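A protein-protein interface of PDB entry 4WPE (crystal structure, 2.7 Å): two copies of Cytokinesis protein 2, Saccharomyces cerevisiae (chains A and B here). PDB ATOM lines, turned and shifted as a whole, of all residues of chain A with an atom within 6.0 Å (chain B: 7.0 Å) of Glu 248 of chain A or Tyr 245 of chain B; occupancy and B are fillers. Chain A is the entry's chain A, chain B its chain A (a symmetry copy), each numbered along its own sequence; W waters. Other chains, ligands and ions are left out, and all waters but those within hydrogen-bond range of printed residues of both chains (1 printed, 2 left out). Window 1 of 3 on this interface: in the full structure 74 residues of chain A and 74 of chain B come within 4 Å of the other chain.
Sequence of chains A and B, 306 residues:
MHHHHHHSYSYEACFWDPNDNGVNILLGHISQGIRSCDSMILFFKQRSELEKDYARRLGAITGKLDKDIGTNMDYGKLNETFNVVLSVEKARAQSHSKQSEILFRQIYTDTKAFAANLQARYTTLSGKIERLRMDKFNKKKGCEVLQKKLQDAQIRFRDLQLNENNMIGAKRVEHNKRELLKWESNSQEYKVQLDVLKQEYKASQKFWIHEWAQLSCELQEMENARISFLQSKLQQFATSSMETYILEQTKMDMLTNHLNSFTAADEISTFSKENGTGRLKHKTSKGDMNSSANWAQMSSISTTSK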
ATOM      1  N   TYR A  54       9.311  12.777 -31.193  1.00  0.00           N
ATOM      2  CA  TYR A  54       8.624  14.032 -30.915  1.00  0.00           C
ATOM      3  C   TYR A  54       9.498  15.217 -31.313  1.00  0.00           C
ATOM      4  O   TYR A  54       9.032  16.145 -31.969  1.00  0.00           O
ATOM      5  CB  TYR A  54       8.241  14.128 -29.438  1.00  0.00           C
ATOM      6  CG  TYR A  54       7.445  15.366 -29.086  1.00  0.00           C
ATOM      7  CD1 TYR A  54       6.071  15.415 -29.285  1.00  0.00           C
ATOM      8  CD2 TYR A  54       8.069  16.486 -28.554  1.00  0.00           C
ATOM      9  CE1 TYR A  54       5.341  16.550 -28.963  1.00  0.00           C
ATOM     10  CE2 TYR A  54       7.350  17.622 -28.232  1.00  0.00           C
ATOM     11  CZ  TYR A  54       5.988  17.650 -28.438  1.00  0.00           C
ATOM     12  OH  TYR A  54       5.277  18.784 -28.114  1.00  0.00           O
ATOM     13  N   VAL A  88      10.754  29.627 -30.102  1.00  0.00           N
ATOM     14  CA  VAL A  88      10.284  28.934 -28.908  1.00  0.00           C
ATOM     15  C   VAL A  88      10.135  27.440 -29.171  1.00  0.00           C
ATOM     16  O   VAL A  88      10.576  26.611 -28.375  1.00  0.00           O
ATOM     17  CB  VAL A  88       8.934  29.505 -28.417  1.00  0.00           C
ATOM     18  CG1 VAL A  88       8.188  28.489 -27.560  1.00  0.00           C
ATOM     19  CG2 VAL A  88       9.148  30.808 -27.660  1.00  0.00           C
ATOM     20  N   GLU A  89       9.531  27.102 -30.306  1.00  0.00           N
ATOM     21  CA  GLU A  89       9.225  25.712 -30.620  1.00  0.00           C
ATOM     22  C   GLU A  89      10.461  24.891 -30.976  1.00  0.00           C
ATOM     23  O   GLU A  89      10.520  23.704 -30.670  1.00  0.00           O
ATOM     24  CB  GLU A  89       8.204  25.640 -31.758  1.00  0.00           C
ATOM     25  CG  GLU A  89       6.805  26.097 -31.362  1.00  0.00           C
ATOM     26  CD  GLU A  89       6.163  25.192 -30.324  1.00  0.00           C
ATOM     27  OE1 GLU A  89       5.631  24.129 -30.708  1.00  0.00           O
ATOM     28  OE2 GLU A  89       6.193  25.542 -29.124  1.00  0.00           O
ATOM     29  N   ARG A  92      12.064  23.886 -27.711  1.00  0.00           N
ATOM     30  CA  ARG A  92      11.430  22.705 -27.134  1.00  0.00           C
ATOM     31  C   ARG A  92      11.929  21.446 -27.827  1.00  0.00           C
ATOM     32  O   ARG A  92      12.245  20.451 -27.173  1.00  0.00           O
ATOM     33  CB  ARG A  92       9.906  22.783 -27.242  1.00  0.00           C
ATOM     34  CG  ARG A  92       9.275  23.909 -26.443  1.00  0.00           C
ATOM     35  CD  ARG A  92       7.795  23.648 -26.183  1.00  0.00           C
ATOM     36  NE  ARG A  92       7.030  23.423 -27.406  1.00  0.00           N
ATOM     37  CZ  ARG A  92       6.573  22.237 -27.800  1.00  0.00           C
ATOM     38  NH1 ARG A  92       6.806  21.154 -27.071  1.00  0.00           N
ATOM     39  NH2 ARG A  92       5.881  22.133 -28.927  1.00  0.00           N
ATOM     40  N   SER A  95      15.155  20.557 -26.665  1.00  0.00           N
ATOM     41  CA  SER A  95      15.064  20.169 -25.263  1.00  0.00           C
ATOM     42  C   SER A  95      14.562  18.737 -25.115  1.00  0.00           C
ATOM     43  O   SER A  95      15.046  17.981 -24.270  1.00  0.00           O
ATOM     44  CB  SER A  95      14.149  21.127 -24.503  1.00  0.00           C
ATOM     45  OG  SER A  95      14.053  20.755 -23.141  1.00  0.00           O
ATOM     46  N   HIS A  96      13.584  18.369 -25.936  1.00  0.00           N
ATOM     47  CA  HIS A  96      13.077  17.002 -25.939  1.00  0.00           C
ATOM     48  C   HIS A  96      14.110  16.058 -26.538  1.00  0.00           C
ATOM     49  O   HIS A  96      14.228  14.907 -26.117  1.00  0.00           O
ATOM     50  CB  HIS A  96      11.763  16.907 -26.713  1.00  0.00           C
ATOM     51  CG  HIS A  96      10.579  17.443 -25.967  1.00  0.00           C
ATOM     52  ND1 HIS A  96       9.572  16.635 -25.496  1.00  0.00           N
ATOM     53  CD2 HIS A  96      10.245  18.710 -25.620  1.00  0.00           C
ATOM     54  CE1 HIS A  96       8.662  17.380 -24.885  1.00  0.00           C
ATOM     55  NE2 HIS A  96       9.049  18.638 -24.947  1.00  0.00           N
ATOM     56  N   GLU A 243      13.514  19.509 -16.101  1.00  0.00           N
ATOM     57  CA  GLU A 243      14.268  20.580 -16.737  1.00  0.00           C
ATOM     58  C   GLU A 243      13.587  21.027 -18.021  1.00  0.00           C
ATOM     59  O   GLU A 243      13.585  22.214 -18.349  1.00  0.00           O
ATOM     60  CB  GLU A 243      15.704  20.134 -17.018  1.00  0.00           C
ATOM     61  CG  GLU A 243      16.619  20.223 -15.806  1.00  0.00           C
ATOM     62  CD  GLU A 243      17.966  19.569 -16.042  1.00  0.00           C
ATOM     63  OE1 GLU A 243      18.048  18.668 -16.902  1.00  0.00           O
ATOM     64  OE2 GLU A 243      18.944  19.958 -15.367  1.00  0.00           O
ATOM     65  N   THR A 244      12.994  20.077 -18.736  1.00  0.00           N
ATOM     66  CA  THR A 244      12.269  20.396 -19.959  1.00  0.00           C
ATOM     67  C   THR A 244      11.015  21.215 -19.672  1.00  0.00           C
ATOM     68  O   THR A 244      10.797  22.262 -20.278  1.00  0.00           O
ATOM     69  CB  THR A 244      11.861  19.129 -20.720  1.00  0.00           C
ATOM     70  OG1 THR A 244      13.030  18.359 -21.023  1.00  0.00           O
ATOM     71  CG2 THR A 244      11.146  19.496 -22.013  1.00  0.00           C
ATOM     72  N   TYR A 245      10.200  20.731 -18.741  1.00  0.00           N
ATOM     73  CA  TYR A 245       8.930  21.370 -18.414  1.00  0.00           C
ATOM     74  C   TYR A 245       9.137  22.787 -17.883  1.00  0.00           C
ATOM     75  O   TYR A 245       8.346  23.686 -18.165  1.00  0.00           O
ATOM     76  CB  TYR A 245       8.163  20.528 -17.390  1.00  0.00           C
ATOM     77  CG  TYR A 245       7.993  19.074 -17.790  1.00  0.00           C
ATOM     78  CD1 TYR A 245       7.816  18.714 -19.120  1.00  0.00           C
ATOM     79  CD2 TYR A 245       8.019  18.061 -16.836  1.00  0.00           C
ATOM     80  CE1 TYR A 245       7.663  17.387 -19.491  1.00  0.00           C
ATOM     81  CE2 TYR A 245       7.868  16.731 -17.197  1.00  0.00           C
ATOM     82  CZ  TYR A 245       7.690  16.401 -18.526  1.00  0.00           C
ATOM     83  OH  TYR A 245       7.541  15.083 -18.894  1.00  0.00           O
ATOM     84  N   ILE A 246      10.206  22.984 -17.119  1.00  0.00           N
ATOM     85  CA  ILE A 246      10.521  24.300 -16.579  1.00  0.00           C
ATOM     86  C   ILE A 246      10.995  25.220 -17.703  1.00  0.00           C
ATOM     87  O   ILE A 246      10.682  26.412 -17.719  1.00  0.00           O
ATOM     88  CB  ILE A 246      11.581  24.209 -15.460  1.00  0.00           C
ATOM     89  CG1 ILE A 246      10.896  23.944 -14.119  1.00  0.00           C
ATOM     90  CG2 ILE A 246      12.380  25.489 -15.354  1.00  0.00           C
ATOM     91  CD1 ILE A 246      11.814  23.386 -13.063  1.00  0.00           C
ATOM     92  N   LEU A 247      11.726  24.654 -18.658  1.00  0.00           N
ATOM     93  CA  LEU A 247      12.159  25.407 -19.831  1.00  0.00           C
ATOM     94  C   LEU A 247      10.973  25.791 -20.708  1.00  0.00           C
ATOM     95  O   LEU A 247      10.854  26.941 -21.136  1.00  0.00           O
ATOM     96  CB  LEU A 247      13.174  24.603 -20.648  1.00  0.00           C
ATOM     97  CG  LEU A 247      13.494  25.124 -22.052  1.00  0.00           C
ATOM     98  CD1 LEU A 247      14.989  25.058 -22.313  1.00  0.00           C
ATOM     99  CD2 LEU A 247      12.739  24.335 -23.119  1.00  0.00           C
ATOM    100  N   GLU A 248      10.103  24.821 -20.976  1.00  0.00           N
ATOM    101  CA  GLU A 248       8.947  25.041 -21.842  1.00  0.00           C
ATOM    102  C   GLU A 248       8.029  26.118 -21.278  1.00  0.00           C
ATOM    103  O   GLU A 248       7.379  26.846 -22.027  1.00  0.00           O
ATOM    104  CB  GLU A 248       8.172  23.736 -22.047  1.00  0.00           C
ATOM    105  CG  GLU A 248       8.948  22.682 -22.825  1.00  0.00           C
ATOM    106  CD  GLU A 248       8.162  21.403 -23.046  1.00  0.00           C
ATOM    107  OE1 GLU A 248       8.017  20.610 -22.087  1.00  0.00           O
ATOM    108  OE2 GLU A 248       7.694  21.187 -24.183  1.00  0.00           O
ATOM    109  N   GLN A 249       7.987  26.221 -19.954  1.00  0.00           N
ATOM    110  CA  GLN A 249       7.195  27.258 -19.310  1.00  0.00           C
ATOM    111  C   GLN A 249       7.798  28.638 -19.569  1.00  0.00           C
ATOM    112  O   GLN A 249       7.084  29.593 -19.866  1.00  0.00           O
ATOM    113  CB  GLN A 249       7.078  26.990 -17.807  1.00  0.00           C
ATOM    114  CG  GLN A 249       6.468  28.137 -17.016  1.00  0.00           C
ATOM    115  CD  GLN A 249       6.231  27.782 -15.561  1.00  0.00           C
ATOM    116  OE1 GLN A 249       6.891  26.903 -15.008  1.00  0.00           O
ATOM    117  NE2 GLN A 249       5.275  28.461 -14.935  1.00  0.00           N
ATOM    118  N   THR A 250       9.121  28.728 -19.471  1.00  0.00           N
ATOM    119  CA  THR A 250       9.830  29.988 -19.668  1.00  0.00           C
ATOM    120  C   THR A 250       9.665  30.502 -21.094  1.00  0.00           C
ATOM    121  O   THR A 250       9.594  31.709 -21.327  1.00  0.00           O
ATOM    122  CB  THR A 250      11.332  29.834 -19.353  1.00  0.00           C
ATOM    123  OG1 THR A 250      11.490  29.254 -18.052  1.00  0.00           O
ATOM    124  CG2 THR A 250      12.033  31.182 -19.383  1.00  0.00           C
ATOM    125  N   LYS A 251       9.598  29.579 -22.046  1.00  0.00           N
ATOM    126  CA  LYS A 251       9.462  29.945 -23.450  1.00  0.00           C
ATOM    127  C   LYS A 251       8.054  30.436 -23.770  1.00  0.00           C
ATOM    128  O   LYS A 251       7.879  31.327 -24.599  1.00  0.00           O
ATOM    129  CB  LYS A 251       9.832  28.763 -24.345  1.00  0.00           C
ATOM    130  CG  LYS A 251      11.287  28.349 -24.225  1.00  0.00           C
ATOM    131  CD  LYS A 251      12.199  29.564 -24.269  1.00  0.00           C
ATOM    132  CE  LYS A 251      13.656  29.165 -24.397  1.00  0.00           C
ATOM    133  NZ  LYS A 251      14.548  30.355 -24.318  1.00  0.00           N
ATOM    134  N   MET A 252       7.054  29.857 -23.114  1.00  0.00           N
ATOM    135  CA  MET A 252       5.679  30.316 -23.287  1.00  0.00           C
ATOM    136  C   MET A 252       5.455  31.618 -22.527  1.00  0.00           C
ATOM    137  O   MET A 252       4.533  32.375 -22.835  1.00  0.00           O
ATOM    138  CB  MET A 252       4.680  29.254 -22.826  1.00  0.00           C
ATOM    139  CG  MET A 252       4.732  27.965 -23.627  1.00  0.00           C
ATOM    140  SD  MET A 252       4.175  28.221 -25.475  1.00  0.00           S
ATOM    141  CE  MET A 252       4.560  26.440 -26.176  1.00  0.00           C
ATOM    142  N   ASP A 253       6.297  31.876 -21.530  1.00  0.00           N
ATOM    143  CA  ASP A 253       6.290  33.171 -20.863  1.00  0.00           C
ATOM    144  C   ASP A 253       6.750  34.234 -21.850  1.00  0.00           C
ATOM    145  O   ASP A 253       6.143  35.298 -21.951  1.00  0.00           O
ATOM    146  CB  ASP A 253       7.186  33.169 -19.622  1.00  0.00           C
ATOM    147  CG  ASP A 253       6.488  32.613 -18.393  1.00  0.00           C
ATOM    148  OD1 ASP A 253       5.248  32.742 -18.296  1.00  0.00           O
ATOM    149  OD2 ASP A 253       7.182  32.054 -17.519  1.00  0.00           O
ATOM    150  N   ARG B  47       0.907  20.678 -35.534  1.00  0.00           N
ATOM    151  CA  ARG B  47       1.153  20.651 -34.097  1.00  0.00           C
ATOM    152  C   ARG B  47       0.061  19.866 -33.363  1.00  0.00           C
ATOM    153  O   ARG B  47       0.345  19.121 -32.427  1.00  0.00           O
ATOM    154  CB  ARG B  47       1.241  22.078 -33.556  1.00  0.00           C
ATOM    155  CG  ARG B  47       1.299  22.186 -32.051  1.00  0.00           C
ATOM    156  CD  ARG B  47       2.686  21.907 -31.522  1.00  0.00           C
ATOM    157  NE  ARG B  47       3.006  22.793 -30.408  1.00  0.00           N
ATOM    158  CZ  ARG B  47       2.636  22.574 -29.151  1.00  0.00           C
ATOM    159  NH1 ARG B  47       1.929  21.496 -28.847  1.00  0.00           N
ATOM    160  NH2 ARG B  47       2.971  23.435 -28.198  1.00  0.00           N
ATOM    161  N   GLU B  51       0.598  16.213 -31.163  1.00  0.00           N
ATOM    162  CA  GLU B  51       0.258  15.985 -29.764  1.00  0.00           C
ATOM    163  C   GLU B  51      -0.648  14.769 -29.597  1.00  0.00           C
ATOM    164  O   GLU B  51      -0.575  14.063 -28.592  1.00  0.00           O
ATOM    165  CB  GLU B  51      -0.414  17.225 -29.168  1.00  0.00           C
ATOM    166  CG  GLU B  51       0.486  18.450 -29.081  1.00  0.00           C
ATOM    167  CD  GLU B  51       1.657  18.260 -28.132  1.00  0.00           C
ATOM    168  OE1 GLU B  51       1.562  17.410 -27.223  1.00  0.00           O
ATOM    169  OE2 GLU B  51       2.677  18.966 -28.293  1.00  0.00           O
ATOM    170  N   SER B  95      -3.211  14.937 -20.708  1.00  0.00           N
ATOM    171  CA  SER B  95      -3.016  16.379 -20.797  1.00  0.00           C
ATOM    172  C   SER B  95      -2.614  16.798 -22.206  1.00  0.00           C
ATOM    173  O   SER B  95      -3.072  17.823 -22.716  1.00  0.00           O
ATOM    174  CB  SER B  95      -1.962  16.838 -19.792  1.00  0.00           C
ATOM    175  OG  SER B  95      -1.765  18.237 -19.874  1.00  0.00           O
ATOM    176  N   HIS B  96      -1.749  16.006 -22.832  1.00  0.00           N
ATOM    177  CA  HIS B  96      -1.352  16.264 -24.210  1.00  0.00           C
ATOM    178  C   HIS B  96      -2.507  15.968 -25.157  1.00  0.00           C
ATOM    179  O   HIS B  96      -2.672  16.639 -26.175  1.00  0.00           O
ATOM    180  CB  HIS B  96      -0.129  15.431 -24.592  1.00  0.00           C
ATOM    181  CG  HIS B  96       1.159  15.948 -24.025  1.00  0.00           C
ATOM    182  ND1 HIS B  96       2.141  16.507 -24.807  1.00  0.00           N
ATOM    183  CD2 HIS B  96       1.620  15.983 -22.752  1.00  0.00           C
ATOM    184  CE1 HIS B  96       3.160  16.868 -24.041  1.00  0.00           C
ATOM    185  NE2 HIS B  96       2.867  16.562 -22.793  1.00  0.00           N
ATOM    186  N   GLN B  99      -4.832  18.817 -24.925  1.00  0.00           N
ATOM    187  CA  GLN B  99      -4.176  19.922 -25.614  1.00  0.00           C
ATOM    188  C   GLN B  99      -4.316  19.776 -27.124  1.00  0.00           C
ATOM    189  O   GLN B  99      -4.530  20.757 -27.838  1.00  0.00           O
ATOM    190  CB  GLN B  99      -2.699  19.992 -25.226  1.00  0.00           C
ATOM    191  CG  GLN B  99      -2.017  21.307 -25.576  1.00  0.00           C
ATOM    192  CD  GLN B  99      -0.505  21.181 -25.621  1.00  0.00           C
ATOM    193  OE1 GLN B  99       0.064  20.730 -26.616  1.00  0.00           O
ATOM    194  NE2 GLN B  99       0.153  21.563 -24.534  1.00  0.00           N
ATOM    195  N   PHE B 237      -3.159  29.601 -27.653  1.00  0.00           N
ATOM    196  CA  PHE B 237      -2.117  28.619 -27.915  1.00  0.00           C
ATOM    197  C   PHE B 237      -1.125  28.550 -26.755  1.00  0.00           C
ATOM    198  O   PHE B 237      -0.874  27.478 -26.203  1.00  0.00           O
ATOM    199  CB  PHE B 237      -1.403  28.969 -29.224  1.00  0.00           C
ATOM    200  CG  PHE B 237      -0.137  28.201 -29.459  1.00  0.00           C
ATOM    201  CD1 PHE B 237      -0.177  26.880 -29.866  1.00  0.00           C
ATOM    202  CD2 PHE B 237       1.096  28.818 -29.312  1.00  0.00           C
ATOM    203  CE1 PHE B 237       0.994  26.177 -30.095  1.00  0.00           C
ATOM    204  CE2 PHE B 237       2.269  28.127 -29.542  1.00  0.00           C
ATOM    205  CZ  PHE B 237       2.219  26.803 -29.933  1.00  0.00           C
ATOM    206  N   ALA B 238      -0.579  29.704 -26.379  1.00  0.00           N
ATOM    207  CA  ALA B 238       0.437  29.784 -25.330  1.00  0.00           C
ATOM    208  C   ALA B 238      -0.118  29.493 -23.936  1.00  0.00           C
ATOM    209  O   ALA B 238       0.645  29.229 -23.011  1.00  0.00           O
ATOM    210  CB  ALA B 238       1.102  31.156 -25.345  1.00  0.00           C
ATOM    211  N   SER B 240      -2.915  27.200 -23.436  1.00  0.00           N
ATOM    212  CA  SER B 240      -3.214  25.772 -23.470  1.00  0.00           C
ATOM    213  C   SER B 240      -1.948  24.946 -23.284  1.00  0.00           C
ATOM    214  O   SER B 240      -1.943  23.956 -22.556  1.00  0.00           O
ATOM    215  CB  SER B 240      -3.893  25.394 -24.786  1.00  0.00           C
ATOM    216  OG  SER B 240      -5.251  25.800 -24.792  1.00  0.00           O
ATOM    217  N   SER B 241      -0.876  25.366 -23.946  1.00  0.00           N
ATOM    218  CA  SER B 241       0.411  24.704 -23.807  1.00  0.00           C
ATOM    219  C   SER B 241       0.953  24.913 -22.399  1.00  0.00           C
ATOM    220  O   SER B 241       1.481  23.988 -21.782  1.00  0.00           O
ATOM    221  CB  SER B 241       1.400  25.229 -24.846  1.00  0.00           C
ATOM    222  OG  SER B 241       0.929  24.988 -26.161  1.00  0.00           O
ATOM    223  N   MET B 242       0.802  26.134 -21.893  1.00  0.00           N
ATOM    224  CA  MET B 242       1.263  26.488 -20.554  1.00  0.00           C
ATOM    225  C   MET B 242       0.632  25.606 -19.483  1.00  0.00           C
ATOM    226  O   MET B 242       1.295  25.203 -18.530  1.00  0.00           O
ATOM    227  CB  MET B 242       0.953  27.955 -20.252  1.00  0.00           C
ATOM    228  CG  MET B 242       1.404  28.406 -18.877  1.00  0.00           C
ATOM    229  SD  MET B 242       3.341  28.350 -18.697  1.00  0.00           S
ATOM    230  CE  MET B 242       3.754  30.089 -19.477  1.00  0.00           C
ATOM    231  N   GLU B 243      -0.654  25.316 -19.645  1.00  0.00           N
ATOM    232  CA  GLU B 243      -1.381  24.520 -18.666  1.00  0.00           C
ATOM    233  C   GLU B 243      -0.793  23.121 -18.568  1.00  0.00           C
ATOM    234  O   GLU B 243      -0.731  22.542 -17.484  1.00  0.00           O
ATOM    235  CB  GLU B 243      -2.866  24.455 -19.022  1.00  0.00           C
ATOM    236  CG  GLU B 243      -3.652  25.684 -18.592  1.00  0.00           C
ATOM    237  CD  GLU B 243      -5.062  25.702 -19.149  1.00  0.00           C
ATOM    238  OE1 GLU B 243      -5.294  25.069 -20.200  1.00  0.00           O
ATOM    239  OE2 GLU B 243      -5.938  26.348 -18.534  1.00  0.00           O
ATOM    240  N   THR B 244      -0.345  22.589 -19.700  1.00  0.00           N
ATOM    241  CA  THR B 244       0.282  21.274 -19.718  1.00  0.00           C
ATOM    242  C   THR B 244       1.616  21.277 -18.981  1.00  0.00           C
ATOM    243  O   THR B 244       1.855  20.441 -18.112  1.00  0.00           O
ATOM    244  CB  THR B 244       0.517  20.781 -21.151  1.00  0.00           C
ATOM    245  OG1 THR B 244      -0.732  20.745 -21.852  1.00  0.00           O
ATOM    246  CG2 THR B 244       1.131  19.387 -21.137  1.00  0.00           C
ATOM    247  N   TYR B 245       2.477  22.226 -19.332  1.00  0.00           N
ATOM    248  CA  TYR B 245       3.818  22.307 -18.763  1.00  0.00           C
ATOM    249  C   TYR B 245       3.772  22.528 -17.253  1.00  0.00           C
ATOM    250  O   TYR B 245       4.599  21.996 -16.513  1.00  0.00           O
ATOM    251  CB  TYR B 245       4.613  23.429 -19.438  1.00  0.00           C
ATOM    252  CG  TYR B 245       4.632  23.346 -20.953  1.00  0.00           C
ATOM    253  CD1 TYR B 245       4.653  22.118 -21.602  1.00  0.00           C
ATOM    254  CD2 TYR B 245       4.619  24.498 -21.734  1.00  0.00           C
ATOM    255  CE1 TYR B 245       4.667  22.036 -22.987  1.00  0.00           C
ATOM    256  CE2 TYR B 245       4.632  24.427 -23.119  1.00  0.00           C
ATOM    257  CZ  TYR B 245       4.657  23.193 -23.738  1.00  0.00           C
ATOM    258  OH  TYR B 245       4.669  23.113 -25.112  1.00  0.00           O
ATOM    259  N   ILE B 246       2.799  23.310 -16.797  1.00  0.00           N
ATOM    260  CA  ILE B 246       2.639  23.570 -15.373  1.00  0.00           C
ATOM    261  C   ILE B 246       2.131  22.312 -14.671  1.00  0.00           C
ATOM    262  O   ILE B 246       2.532  22.011 -13.545  1.00  0.00           O
ATOM    263  CB  ILE B 246       1.687  24.760 -15.123  1.00  0.00           C
ATOM    264  CG1 ILE B 246       2.474  26.070 -15.162  1.00  0.00           C
ATOM    265  CG2 ILE B 246       1.002  24.644 -13.779  1.00  0.00           C
ATOM    266  CD1 ILE B 246       1.621  27.290 -15.393  1.00  0.00           C
ATOM    267  N   LEU B 247       1.271  21.563 -15.353  1.00  0.00           N
ATOM    268  CA  LEU B 247       0.787  20.290 -14.828  1.00  0.00           C
ATOM    269  C   LEU B 247       1.910  19.262 -14.755  1.00  0.00           C
ATOM    270  O   LEU B 247       2.076  18.584 -13.738  1.00  0.00           O
ATOM    271  CB  LEU B 247      -0.360  19.750 -15.687  1.00  0.00           C
ATOM    272  CG  LEU B 247      -0.772  18.294 -15.447  1.00  0.00           C
ATOM    273  CD1 LEU B 247      -2.285  18.170 -15.423  1.00  0.00           C
ATOM    274  CD2 LEU B 247      -0.185  17.372 -16.512  1.00  0.00           C
ATOM    275  N   GLU B 248       2.674  19.147 -15.838  1.00  0.00           N
ATOM    276  CA  GLU B 248       3.754  18.169 -15.917  1.00  0.00           C
ATOM    277  C   GLU B 248       4.802  18.410 -14.838  1.00  0.00           C
ATOM    278  O   GLU B 248       5.432  17.472 -14.351  1.00  0.00           O
ATOM    279  CB  GLU B 248       4.405  18.196 -17.304  1.00  0.00           C
ATOM    280  CG  GLU B 248       3.479  17.730 -18.420  1.00  0.00           C
ATOM    281  CD  GLU B 248       4.141  17.736 -19.786  1.00  0.00           C
ATOM    282  OE1 GLU B 248       4.315  18.831 -20.368  1.00  0.00           O
ATOM    283  OE2 GLU B 248       4.479  16.641 -20.282  1.00  0.00           O
ATOM    284  N   GLN B 249       4.978  19.672 -14.461  1.00  0.00           N
ATOM    285  CA  GLN B 249       5.906  20.010 -13.392  1.00  0.00           C
ATOM    286  C   GLN B 249       5.388  19.502 -12.047  1.00  0.00           C
ATOM    287  O   GLN B 249       6.142  18.948 -11.250  1.00  0.00           O
ATOM    288  CB  GLN B 249       6.144  21.522 -13.345  1.00  0.00           C
ATOM    289  CG  GLN B 249       6.914  21.993 -12.120  1.00  0.00           C
ATOM    290  CD  GLN B 249       7.261  23.468 -12.180  1.00  0.00           C
ATOM    291  OE1 GLN B 249       6.590  24.249 -12.854  1.00  0.00           O
ATOM    292  NE2 GLN B 249       8.321  23.855 -11.478  1.00  0.00           N
ATOM    293  N   THR B 250       4.092  19.679 -11.812  1.00  0.00           N
ATOM    294  CA  THR B 250       3.466  19.265 -10.561  1.00  0.00           C
ATOM    295  C   THR B 250       3.532  17.753 -10.378  1.00  0.00           C
ATOM    296  O   THR B 250       3.673  17.255  -9.261  1.00  0.00           O
ATOM    297  CB  THR B 250       1.993  19.720 -10.500  1.00  0.00           C
ATOM    298  OG1 THR B 250       1.916  21.125 -10.773  1.00  0.00           O
ATOM    299  CG2 THR B 250       1.397  19.450  -9.129  1.00  0.00           C
HETATM  300  O   HOH W   1       3.409  20.736 -26.109  1.00  0.00           O
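The backbone carbonyl oxygen (O) of Phe 237 of chain B is in hydrogen-bond range of the side-chain hydroxyl (OG) of Ser 241 of chain B. The backbone carbonyl oxygen (O) of Ile 246 of chain A lies within hydrogen-bond range of the side-chain hydroxyl (OG1) of Thr 250 of chain A. The side-chain hydroxyl (OG1) of Thr 250 of chain B lies within hydrogen-bond range of the backbone carbonyl oxygen (O) of Ile 246 of chain B.
Of the 18 printed residues of chain B, 8 touch a printed residue of chain A. Printed residues of chain B that touch a printed residue of chain A: Arg 47, Glu 51, Ser 241, Met 242, Tyr 245, Ile 246, Glu 248 and Gln 249. Hydrophobic or aromatic side chains of chain B that line the printed part of chain A: Met 242, Tyr 245 and Ile 246. Among the printed residues, 16 pairs touch across the chains. Among the printed residues, Asp or Glu carboxylates within 4 Å of a Lys or Arg side-chain nitrogen of the other chain: Glu 89 of chain A with Arg 47 of chain B (3.0 Å).
Water W1 lies within hydrogen-bond range of OH of Tyr 245 of chain B, OE2 of Glu 51 of chain B, NH1 of Arg 47 of chain B, OH of Tyr 54 of chain A and OE1 of Gln 99 of chain B.
Tyr 245 of chain B touches its own counterpart, Tyr 245 of chain A. Tyr 245 of chain A touches Glu 248 of chain B, and with the chains exchanged Glu 248 of chain A touches Tyr 245 of chain B. Ile 246 of chain A touches Gln 249 of chain B, and with the chains exchanged Gln 249 of chain A touches Ile 246 of chain B. Gln 249 of chain A touches its own counterpart, Gln 249 of chain B.
Among the printed residues, pairs that only touch across the chains: Tyr 245 of chain A with Tyr 245 of chain B, Tyr 245 of chain A with Glu 248 of chain B, Ile 246 of chain A with Gln 249 of chain B, Glu 248 of chain A with Tyr 245 of chain B, Gln 249 of chain A with Met 242 of chain B, Gln 249 of chain A with Ile 246 of chain B, Met 252 of chain A with Arg 47 of chain B, Met 252 of chain A with Ser 241 of chain B, Met 252 of chain A with Met 242 of chain B, Met 252 of chain A with Tyr 245 of chain B and Asp 253 of chain A with Met 242 of chain B.
Glu 248 of chain A touches just one residue of chain B: Tyr 245. Tyr 245 of chain B touches just these residues of chain A: Arg 92 (3.3 Å), Tyr 245 (3.95 Å), Glu 248 (3.4 Å) and Met 252 (3.5 Å). Printed residues of chain A within 4 Å of Glu 248 of chain B: Tyr 245 (3.4 Å). Printed residues of chain B within 4 Å of Ile 246 of chain A: Gln 249. The nearest residue of chain A that does not touch Tyr 245 of chain B is Gln 249 of chain A (4.2 Å).
The guanidinium group of Arg 47 of chain B sits close to the guanidinium group of Arg 92 of chain A (3.3 Å). OE1 of Glu 89 of chain A lies within salt-bridge range of NE of Arg 47 of chain B. OE1 of Gln 249 of chain B lies close to OE1 of Gln 249 of chain A (3.4 Å). NE of Arg 92 of chain A lies within hydrogen-bond range of OH of Tyr 245 of chain B (3.3 Å). The side-chain hydroxyl of Tyr 54 of chain A sits at hydrogen-bond distance from the side-chain carboxylate of Glu 51 of chain B, 2.6 Å away.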
